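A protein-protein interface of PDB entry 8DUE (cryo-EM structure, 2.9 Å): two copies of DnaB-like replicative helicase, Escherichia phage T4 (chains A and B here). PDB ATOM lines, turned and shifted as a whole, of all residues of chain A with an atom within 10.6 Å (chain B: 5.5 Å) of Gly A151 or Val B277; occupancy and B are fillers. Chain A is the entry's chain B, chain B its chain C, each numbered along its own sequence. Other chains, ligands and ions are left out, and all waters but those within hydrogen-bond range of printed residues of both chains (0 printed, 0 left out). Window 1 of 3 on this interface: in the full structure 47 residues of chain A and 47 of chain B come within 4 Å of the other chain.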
ATOM      1  N   SER A 148      33.674  -1.227 -10.178  1.00  0.00           N
ATOM      2  CA  SER A 148      32.268  -1.131 -10.566  1.00  0.00           C
ATOM      3  C   SER A 148      31.741  -2.541 -10.801  1.00  0.00           C
ATOM      4  O   SER A 148      31.952  -3.119 -11.872  1.00  0.00           O
ATOM      5  CB  SER A 148      32.097  -0.265 -11.809  1.00  0.00           C
ATOM      6  OG  SER A 148      32.754  -0.846 -12.923  1.00  0.00           O
ATOM      7  N   TYR A 149      31.058  -3.093  -9.803  1.00  0.00           N
ATOM      8  CA  TYR A 149      30.434  -4.401  -9.915  1.00  0.00           C
ATOM      9  C   TYR A 149      28.949  -4.292  -9.603  1.00  0.00           C
ATOM     10  O   TYR A 149      28.550  -3.610  -8.655  1.00  0.00           O
ATOM     11  CB  TYR A 149      31.083  -5.418  -8.976  1.00  0.00           C
ATOM     12  CG  TYR A 149      30.385  -6.757  -8.978  1.00  0.00           C
ATOM     13  CD1 TYR A 149      30.423  -7.578 -10.095  1.00  0.00           C
ATOM     14  CD2 TYR A 149      29.686  -7.200  -7.865  1.00  0.00           C
ATOM     15  CE1 TYR A 149      29.785  -8.803 -10.105  1.00  0.00           C
ATOM     16  CE2 TYR A 149      29.045  -8.424  -7.864  1.00  0.00           C
ATOM     17  CZ  TYR A 149      29.098  -9.222  -8.987  1.00  0.00           C
ATOM     18  OH  TYR A 149      28.462 -10.441  -8.993  1.00  0.00           O
ATOM     19  N   VAL A 150      28.138  -4.971 -10.413  1.00  0.00           N
ATOM     20  CA  VAL A 150      26.700  -5.048 -10.214  1.00  0.00           C
ATOM     21  C   VAL A 150      26.299  -6.515 -10.243  1.00  0.00           C
ATOM     22  O   VAL A 150      26.984  -7.360 -10.821  1.00  0.00           O
ATOM     23  CB  VAL A 150      25.914  -4.249 -11.274  1.00  0.00           C
ATOM     24  CG1 VAL A 150      26.254  -2.770 -11.181  1.00  0.00           C
ATOM     25  CG2 VAL A 150      26.215  -4.780 -12.665  1.00  0.00           C
ATOM     26  N   GLY A 151      25.173  -6.812  -9.602  1.00  0.00           N
ATOM     27  CA  GLY A 151      24.720  -8.184  -9.527  1.00  0.00           C
ATOM     28  C   GLY A 151      24.372  -8.749 -10.890  1.00  0.00           C
ATOM     29  O   GLY A 151      23.918  -8.041 -11.790  1.00  0.00           O
ATOM     30  N   HIS A 152      24.594 -10.049 -11.041  1.00  0.00           N
ATOM     31  CA  HIS A 152      24.302 -10.715 -12.299  1.00  0.00           C
ATOM     32  C   HIS A 152      22.800 -10.910 -12.456  1.00  0.00           C
ATOM     33  O   HIS A 152      22.071 -11.106 -11.480  1.00  0.00           O
ATOM     34  CB  HIS A 152      25.016 -12.065 -12.376  1.00  0.00           C
ATOM     35  CG  HIS A 152      24.342 -13.151 -11.597  1.00  0.00           C
ATOM     36  ND1 HIS A 152      23.742 -12.930 -10.377  1.00  0.00           N
ATOM     37  CD2 HIS A 152      24.166 -14.465 -11.871  1.00  0.00           C
ATOM     38  CE1 HIS A 152      23.229 -14.062  -9.930  1.00  0.00           C
ATOM     39  NE2 HIS A 152      23.473 -15.009 -10.817  1.00  0.00           N
ATOM     40  N   ASP A 153      22.340 -10.853 -13.702  1.00  0.00           N
ATOM     41  CA  ASP A 153      20.923 -10.976 -13.997  1.00  0.00           C
ATOM     42  C   ASP A 153      20.517 -12.443 -14.080  1.00  0.00           C
ATOM     43  O   ASP A 153      21.332 -13.322 -14.369  1.00  0.00           O
ATOM     44  CB  ASP A 153      20.575 -10.257 -15.299  1.00  0.00           C
ATOM     45  CG  ASP A 153      20.942  -8.789 -15.261  1.00  0.00           C
ATOM     46  OD1 ASP A 153      21.672  -8.386 -14.332  1.00  0.00           O
ATOM     47  OD2 ASP A 153      20.499  -8.037 -16.153  1.00  0.00           O
ATOM     48  N   TRP A 154      19.232 -12.694 -13.820  1.00  0.00           N
ATOM     49  CA  TRP A 154      18.747 -14.064 -13.712  1.00  0.00           C
ATOM     50  C   TRP A 154      18.703 -14.763 -15.063  1.00  0.00           C
ATOM     51  O   TRP A 154      18.765 -15.996 -15.126  1.00  0.00           O
ATOM     52  CB  TRP A 154      17.364 -14.070 -13.063  1.00  0.00           C
ATOM     53  CG  TRP A 154      16.789 -15.435 -12.845  1.00  0.00           C
ATOM     54  CD1 TRP A 154      17.200 -16.360 -11.934  1.00  0.00           C
ATOM     55  CD2 TRP A 154      15.681 -16.021 -13.539  1.00  0.00           C
ATOM     56  NE1 TRP A 154      16.426 -17.491 -12.024  1.00  0.00           N
ATOM     57  CE2 TRP A 154      15.484 -17.306 -13.001  1.00  0.00           C
ATOM     58  CE3 TRP A 154      14.840 -15.583 -14.565  1.00  0.00           C
ATOM     59  CZ2 TRP A 154      14.481 -18.160 -13.454  1.00  0.00           C
ATOM     60  CZ3 TRP A 154      13.845 -16.433 -15.014  1.00  0.00           C
ATOM     61  CH2 TRP A 154      13.674 -17.706 -14.459  1.00  0.00           C
ATOM     62  N   MET A 155      18.600 -14.003 -16.152  1.00  0.00           N
ATOM     63  CA  MET A 155      18.460 -14.581 -17.482  1.00  0.00           C
ATOM     64  C   MET A 155      19.651 -14.300 -18.387  1.00  0.00           C
ATOM     65  O   MET A 155      19.999 -15.142 -19.219  1.00  0.00           O
ATOM     66  CB  MET A 155      17.178 -14.064 -18.145  1.00  0.00           C
ATOM     67  CG  MET A 155      16.842 -14.709 -19.482  1.00  0.00           C
ATOM     68  SD  MET A 155      17.554 -13.845 -20.897  1.00  0.00           S
ATOM     69  CE  MET A 155      16.778 -12.240 -20.739  1.00  0.00           C
ATOM     70  N   ASP A 156      20.286 -13.133 -18.246  1.00  0.00           N
ATOM     71  CA  ASP A 156      21.361 -12.759 -19.160  1.00  0.00           C
ATOM     72  C   ASP A 156      22.537 -13.724 -19.072  1.00  0.00           C
ATOM     73  O   ASP A 156      23.106 -14.115 -20.097  1.00  0.00           O
ATOM     74  CB  ASP A 156      21.819 -11.331 -18.869  1.00  0.00           C
ATOM     75  CG  ASP A 156      20.691 -10.326 -18.976  1.00  0.00           C
ATOM     76  OD1 ASP A 156      19.536 -10.746 -19.197  1.00  0.00           O
ATOM     77  OD2 ASP A 156      20.962  -9.115 -18.840  1.00  0.00           O
ATOM     78  N   ASP A 157      22.916 -14.119 -17.860  1.00  0.00           N
ATOM     79  CA  ASP A 157      24.104 -14.934 -17.629  1.00  0.00           C
ATOM     80  C   ASP A 157      23.755 -16.295 -17.037  1.00  0.00           C
ATOM     81  O   ASP A 157      24.426 -16.778 -16.124  1.00  0.00           O
ATOM     82  CB  ASP A 157      25.083 -14.202 -16.716  1.00  0.00           C
ATOM     83  CG  ASP A 157      25.179 -12.723 -17.027  1.00  0.00           C
ATOM     84  OD1 ASP A 157      25.076 -12.351 -18.214  1.00  0.00           O
ATOM     85  OD2 ASP A 157      25.355 -11.928 -16.081  1.00  0.00           O
ATOM     86  N   ARG A 161      25.601 -19.672 -14.570  1.00  0.00           N
ATOM     87  CA  ARG A 161      24.917 -20.261 -13.425  1.00  0.00           C
ATOM     88  C   ARG A 161      24.762 -21.767 -13.592  1.00  0.00           C
ATOM     89  O   ARG A 161      24.924 -22.527 -12.631  1.00  0.00           O
ATOM     90  CB  ARG A 161      23.558 -19.591 -13.223  1.00  0.00           C
ATOM     91  CG  ARG A 161      23.627 -18.068 -13.166  1.00  0.00           C
ATOM     92  CD  ARG A 161      22.303 -17.440 -12.754  1.00  0.00           C
ATOM     93  NE  ARG A 161      21.224 -17.725 -13.692  1.00  0.00           N
ATOM     94  CZ  ARG A 161      20.323 -18.682 -13.524  1.00  0.00           C
ATOM     95  NH1 ARG A 161      20.350 -19.476 -12.467  1.00  0.00           N
ATOM     96  NH2 ARG A 161      19.371 -18.846 -14.438  1.00  0.00           N
ATOM     97  N   TYR A 165      26.142 -24.858 -11.379  1.00  0.00           N
ATOM     98  CA  TYR A 165      25.327 -25.985 -10.930  1.00  0.00           C
ATOM     99  C   TYR A 165      25.983 -27.315 -11.283  1.00  0.00           C
ATOM    100  O   TYR A 165      26.015 -28.242 -10.466  1.00  0.00           O
ATOM    101  CB  TYR A 165      23.933 -25.917 -11.554  1.00  0.00           C
ATOM    102  CG  TYR A 165      23.107 -24.720 -11.159  1.00  0.00           C
ATOM    103  CD1 TYR A 165      23.106 -24.242  -9.857  1.00  0.00           C
ATOM    104  CD2 TYR A 165      22.326 -24.064 -12.097  1.00  0.00           C
ATOM    105  CE1 TYR A 165      22.347 -23.144  -9.503  1.00  0.00           C
ATOM    106  CE2 TYR A 165      21.568 -22.965 -11.754  1.00  0.00           C
ATOM    107  CZ  TYR A 165      21.583 -22.512 -10.458  1.00  0.00           C
ATOM    108  OH  TYR A 165      20.827 -21.420 -10.119  1.00  0.00           O
ATOM    109  N   TYR B 223      17.059  -7.149  -6.097  1.00  0.00           N
ATOM    110  CA  TYR B 223      17.250  -8.018  -4.949  1.00  0.00           C
ATOM    111  C   TYR B 223      18.575  -7.674  -4.286  1.00  0.00           C
ATOM    112  O   TYR B 223      19.599  -7.540  -4.962  1.00  0.00           O
ATOM    113  CB  TYR B 223      17.224  -9.483  -5.378  1.00  0.00           C
ATOM    114  CG  TYR B 223      16.848 -10.447  -4.285  1.00  0.00           C
ATOM    115  CD1 TYR B 223      17.686 -10.666  -3.206  1.00  0.00           C
ATOM    116  CD2 TYR B 223      15.662 -11.156  -4.343  1.00  0.00           C
ATOM    117  CE1 TYR B 223      17.346 -11.554  -2.209  1.00  0.00           C
ATOM    118  CE2 TYR B 223      15.316 -12.043  -3.356  1.00  0.00           C
ATOM    119  CZ  TYR B 223      16.160 -12.240  -2.292  1.00  0.00           C
ATOM    120  OH  TYR B 223      15.810 -13.129  -1.305  1.00  0.00           O
ATOM    121  N   SER B 225      20.704  -9.217  -1.294  1.00  0.00           N
ATOM    122  CA  SER B 225      20.866 -10.304  -0.342  1.00  0.00           C
ATOM    123  C   SER B 225      21.993  -9.962   0.622  1.00  0.00           C
ATOM    124  O   SER B 225      23.117  -9.678   0.196  1.00  0.00           O
ATOM    125  CB  SER B 225      21.155 -11.617  -1.065  1.00  0.00           C
ATOM    126  OG  SER B 225      21.264 -12.686  -0.144  1.00  0.00           O
ATOM    127  N   ALA B 229      24.656 -15.699  -1.070  1.00  0.00           N
ATOM    128  CA  ALA B 229      25.365 -15.206  -2.238  1.00  0.00           C
ATOM    129  C   ALA B 229      24.413 -15.057  -3.423  1.00  0.00           C
ATOM    130  O   ALA B 229      23.271 -15.523  -3.407  1.00  0.00           O
ATOM    131  CB  ALA B 229      26.518 -16.142  -2.599  1.00  0.00           C
ATOM    132  N   GLU B 230      24.909 -14.388  -4.466  1.00  0.00           N
ATOM    133  CA  GLU B 230      24.101 -14.162  -5.660  1.00  0.00           C
ATOM    134  C   GLU B 230      23.703 -15.477  -6.317  1.00  0.00           C
ATOM    135  O   GLU B 230      22.571 -15.628  -6.791  1.00  0.00           O
ATOM    136  CB  GLU B 230      24.868 -13.281  -6.642  1.00  0.00           C
ATOM    137  CG  GLU B 230      25.366 -11.988  -6.028  1.00  0.00           C
ATOM    138  CD  GLU B 230      26.453 -11.331  -6.849  1.00  0.00           C
ATOM    139  OE1 GLU B 230      26.751 -11.829  -7.955  1.00  0.00           O
ATOM    140  OE2 GLU B 230      27.015 -10.318  -6.387  1.00  0.00           O
ATOM    141  N   CYS B 233      20.712 -17.067  -4.438  1.00  0.00           N
ATOM    142  CA  CYS B 233      19.440 -16.410  -4.725  1.00  0.00           C
ATOM    143  C   CYS B 233      18.961 -16.725  -6.135  1.00  0.00           C
ATOM    144  O   CYS B 233      17.766 -16.969  -6.353  1.00  0.00           O
ATOM    145  CB  CYS B 233      19.568 -14.903  -4.522  1.00  0.00           C
ATOM    146  SG  CYS B 233      19.874 -14.422  -2.810  1.00  0.00           S
ATOM    147  N   ALA B 234      19.875 -16.720  -7.107  1.00  0.00           N
ATOM    148  CA  ALA B 234      19.505 -17.119  -8.459  1.00  0.00           C
ATOM    149  C   ALA B 234      18.998 -18.554  -8.482  1.00  0.00           C
ATOM    150  O   ALA B 234      18.062 -18.879  -9.218  1.00  0.00           O
ATOM    151  CB  ALA B 234      20.695 -16.948  -9.401  1.00  0.00           C
ATOM    152  N   ILE B 237      15.453 -18.575  -7.196  1.00  0.00           N
ATOM    153  CA  ILE B 237      14.572 -18.070  -8.246  1.00  0.00           C
ATOM    154  C   ILE B 237      14.344 -19.138  -9.311  1.00  0.00           C
ATOM    155  O   ILE B 237      13.225 -19.316  -9.802  1.00  0.00           O
ATOM    156  CB  ILE B 237      15.141 -16.773  -8.851  1.00  0.00           C
ATOM    157  CG1 ILE B 237      15.263 -15.695  -7.774  1.00  0.00           C
ATOM    158  CG2 ILE B 237      14.247 -16.264  -9.961  1.00  0.00           C
ATOM    159  CD1 ILE B 237      13.951 -15.332  -7.126  1.00  0.00           C
ATOM    160  N   LEU B 275      15.379  -9.454 -13.531  1.00  0.00           N
ATOM    161  CA  LEU B 275      15.787  -9.676 -12.152  1.00  0.00           C
ATOM    162  C   LEU B 275      17.301  -9.582 -12.046  1.00  0.00           C
ATOM    163  O   LEU B 275      18.022 -10.088 -12.910  1.00  0.00           O
ATOM    164  CB  LEU B 275      15.306 -11.048 -11.651  1.00  0.00           C
ATOM    165  CG  LEU B 275      15.149 -11.308 -10.151  1.00  0.00           C
ATOM    166  CD1 LEU B 275      14.233 -12.498  -9.926  1.00  0.00           C
ATOM    167  CD2 LEU B 275      16.485 -11.555  -9.485  1.00  0.00           C
ATOM    168  N   ILE B 276      17.775  -8.928 -10.989  1.00  0.00           N
ATOM    169  CA  ILE B 276      19.189  -8.909 -10.645  1.00  0.00           C
ATOM    170  C   ILE B 276      19.318  -9.254  -9.171  1.00  0.00           C
ATOM    171  O   ILE B 276      18.374  -9.095  -8.393  1.00  0.00           O
ATOM    172  CB  ILE B 276      19.858  -7.548 -10.939  1.00  0.00           C
ATOM    173  CG1 ILE B 276      19.443  -6.514  -9.898  1.00  0.00           C
ATOM    174  CG2 ILE B 276      19.503  -7.060 -12.330  1.00  0.00           C
ATOM    175  CD1 ILE B 276      20.204  -5.231 -10.013  1.00  0.00           C
ATOM    176  N   VAL B 277      20.496  -9.739  -8.787  1.00  0.00           N
ATOM    177  CA  VAL B 277      20.777 -10.107  -7.406  1.00  0.00           C
ATOM    178  C   VAL B 277      22.123  -9.520  -7.019  1.00  0.00           C
ATOM    179  O   VAL B 277      23.163  -9.977  -7.505  1.00  0.00           O
ATOM    180  CB  VAL B 277      20.782 -11.628  -7.197  1.00  0.00           C
ATOM    181  CG1 VAL B 277      21.207 -11.951  -5.779  1.00  0.00           C
ATOM    182  CG2 VAL B 277      19.415 -12.213  -7.486  1.00  0.00           C
ATOM    183  N   LYS B 278      22.108  -8.529  -6.136  1.00  0.00           N
ATOM    184  CA  LYS B 278      23.320  -7.925  -5.606  1.00  0.00           C
ATOM    185  C   LYS B 278      23.528  -8.399  -4.176  1.00  0.00           C
ATOM    186  O   LYS B 278      22.643  -8.234  -3.332  1.00  0.00           O
ATOM    187  CB  LYS B 278      23.237  -6.400  -5.647  1.00  0.00           C
ATOM    188  CG  LYS B 278      24.224  -5.706  -4.727  1.00  0.00           C
ATOM    189  CD  LYS B 278      25.656  -5.898  -5.193  1.00  0.00           C
ATOM    190  CE  LYS B 278      25.894  -5.214  -6.527  1.00  0.00           C
ATOM    191  NZ  LYS B 278      27.327  -5.258  -6.926  1.00  0.00           N
ATOM    192  N   GLN B 279      24.693  -8.977  -3.907  1.00  0.00           N
ATOM    193  CA  GLN B 279      25.027  -9.458  -2.575  1.00  0.00           C
ATOM    194  C   GLN B 279      25.965  -8.478  -1.888  1.00  0.00           C
ATOM    195  O   GLN B 279      26.865  -7.916  -2.518  1.00  0.00           O
ATOM    196  CB  GLN B 279      25.678 -10.839  -2.627  1.00  0.00           C
ATOM    197  CG  GLN B 279      25.925 -11.443  -1.256  1.00  0.00           C
ATOM    198  CD  GLN B 279      27.173 -12.297  -1.209  1.00  0.00           C
ATOM    199  OE1 GLN B 279      27.584 -12.755  -0.143  1.00  0.00           O
ATOM    200  NE2 GLN B 279      27.788 -12.512  -2.365  1.00  0.00           N
ATOM    201  N   LEU B 293      25.544   2.532  -7.171  1.00  0.00           N
ATOM    202  CA  LEU B 293      25.679   1.496  -8.233  1.00  0.00           C
ATOM    203  C   LEU B 293      24.456   1.531  -9.155  1.00  0.00           C
ATOM    204  O   LEU B 293      24.652   1.437 -10.381  1.00  0.00           O
ATOM    205  CB  LEU B 293      25.840   0.116  -7.584  1.00  0.00           C
ATOM    206  CG  LEU B 293      24.556  -0.695  -7.415  1.00  0.00           C
ATOM    207  CD1 LEU B 293      24.833  -2.184  -7.531  1.00  0.00           C
ATOM    208  CD2 LEU B 293      23.874  -0.376  -6.094  1.00  0.00           C
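No position is printed for both chains.
Of the 17 pairs that touch across the chains among the printed residues, none has its exchanged pair printed and touching as well.
Printed residues of chain B within 4 Å of Tyr A149: Glu B230 (2.4 Å) and Lys B278 (2.7 Å).
Gly A151 touches just these residues of chain B: Val B277 and Lys B278.
Glu B230 touches two residues of chain A.
No residue of chain A comes within 4 Å of Cys B233.
Val B277 touches two residues of chain A.
Lys B278 touches just these residues of chain A: Tyr A149 (2.7 Å), Val A150 (3.4 Å) and Gly A151 (3.5 Å).
Of the printed residues of chain A, Leu B293 touches Val A150 (3.96 Å).
The nearest residue of chain B that does not touch Gly A151 is Ile B276 (4.2 Å).
The nearest printed residue of chain A that does not touch Leu B293 is Tyr A149 (4.1 Å).
Hydrophobic or aromatic side chains of chain A that line the printed part of chain B: Tyr A149, Val A150, His A152, Trp A154 and Tyr A165.
Along chain A the printed residues that touch a printed residue of chain B span positions 149 to 165.
Hydrophobic or aromatic side chains of chain B within 4 Å of the printed part of chain A: Ala B234, Ile B237, Leu B275, Ile B276 and Leu B293.
Among the printed residues, 17 pairs touch across the chains.
Val A150 touches Lys B278.
Leu B293 touches Val A150.
Gly A151 touches Val B277.
CB of Ala B234 touches NE2 of His A152, at 3.7 Å.
O of His A152 touches CA of Ile B276, 3.7 Å away.
Asp A153 touches Leu B275 (CA to O, 3.2 Å).
Asp A153 touches Ile B276.
Ala B234 touches Trp A154 (O to NE1, 3.5 Å).
CB of Ala B234 touches CD of Arg A161, at 3.8 Å.
C of Ala B234 touches OH of Tyr A165 (3.8 Å).
The backbone NH of Tyr B223 lies close to the backbone carbonyl oxygen of Ile B276, at 3.3 Å.
NH1 of Arg A161 lies within hydrogen-bond range of OH of Tyr A165, 3.1 Å away.
O of Trp A154 lies within hydrogen-bond range of NH2 of Arg A161, at 3.0 Å.
The backbone carbonyl oxygen of Tyr B223 lies within hydrogen-bond range of the backbone NH of Lys B278 (2.9 Å).
The backbone carbonyl oxygen (O) of Lys B278 sits at hydrogen-bond distance from the backbone NH (N) of Ser B225 (3.0 Å).
The backbone carbonyl oxygen (O) of His A152 sits at hydrogen-bond distance from the backbone NH (N) of Val B277 (3.4 Å).
NZ of Lys B278 is in hydrogen-bond range of O of Tyr A149.
The side-chain carboxylate (OE1) of Glu B230 sits at hydrogen-bond distance from the side-chain hydroxyl (OH) of Tyr A149 (2.4 Å).
The backbone NH (N) of Trp A154 sits at hydrogen-bond distance from the backbone carbonyl oxygen (O) of Leu B275 (3.0 Å).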
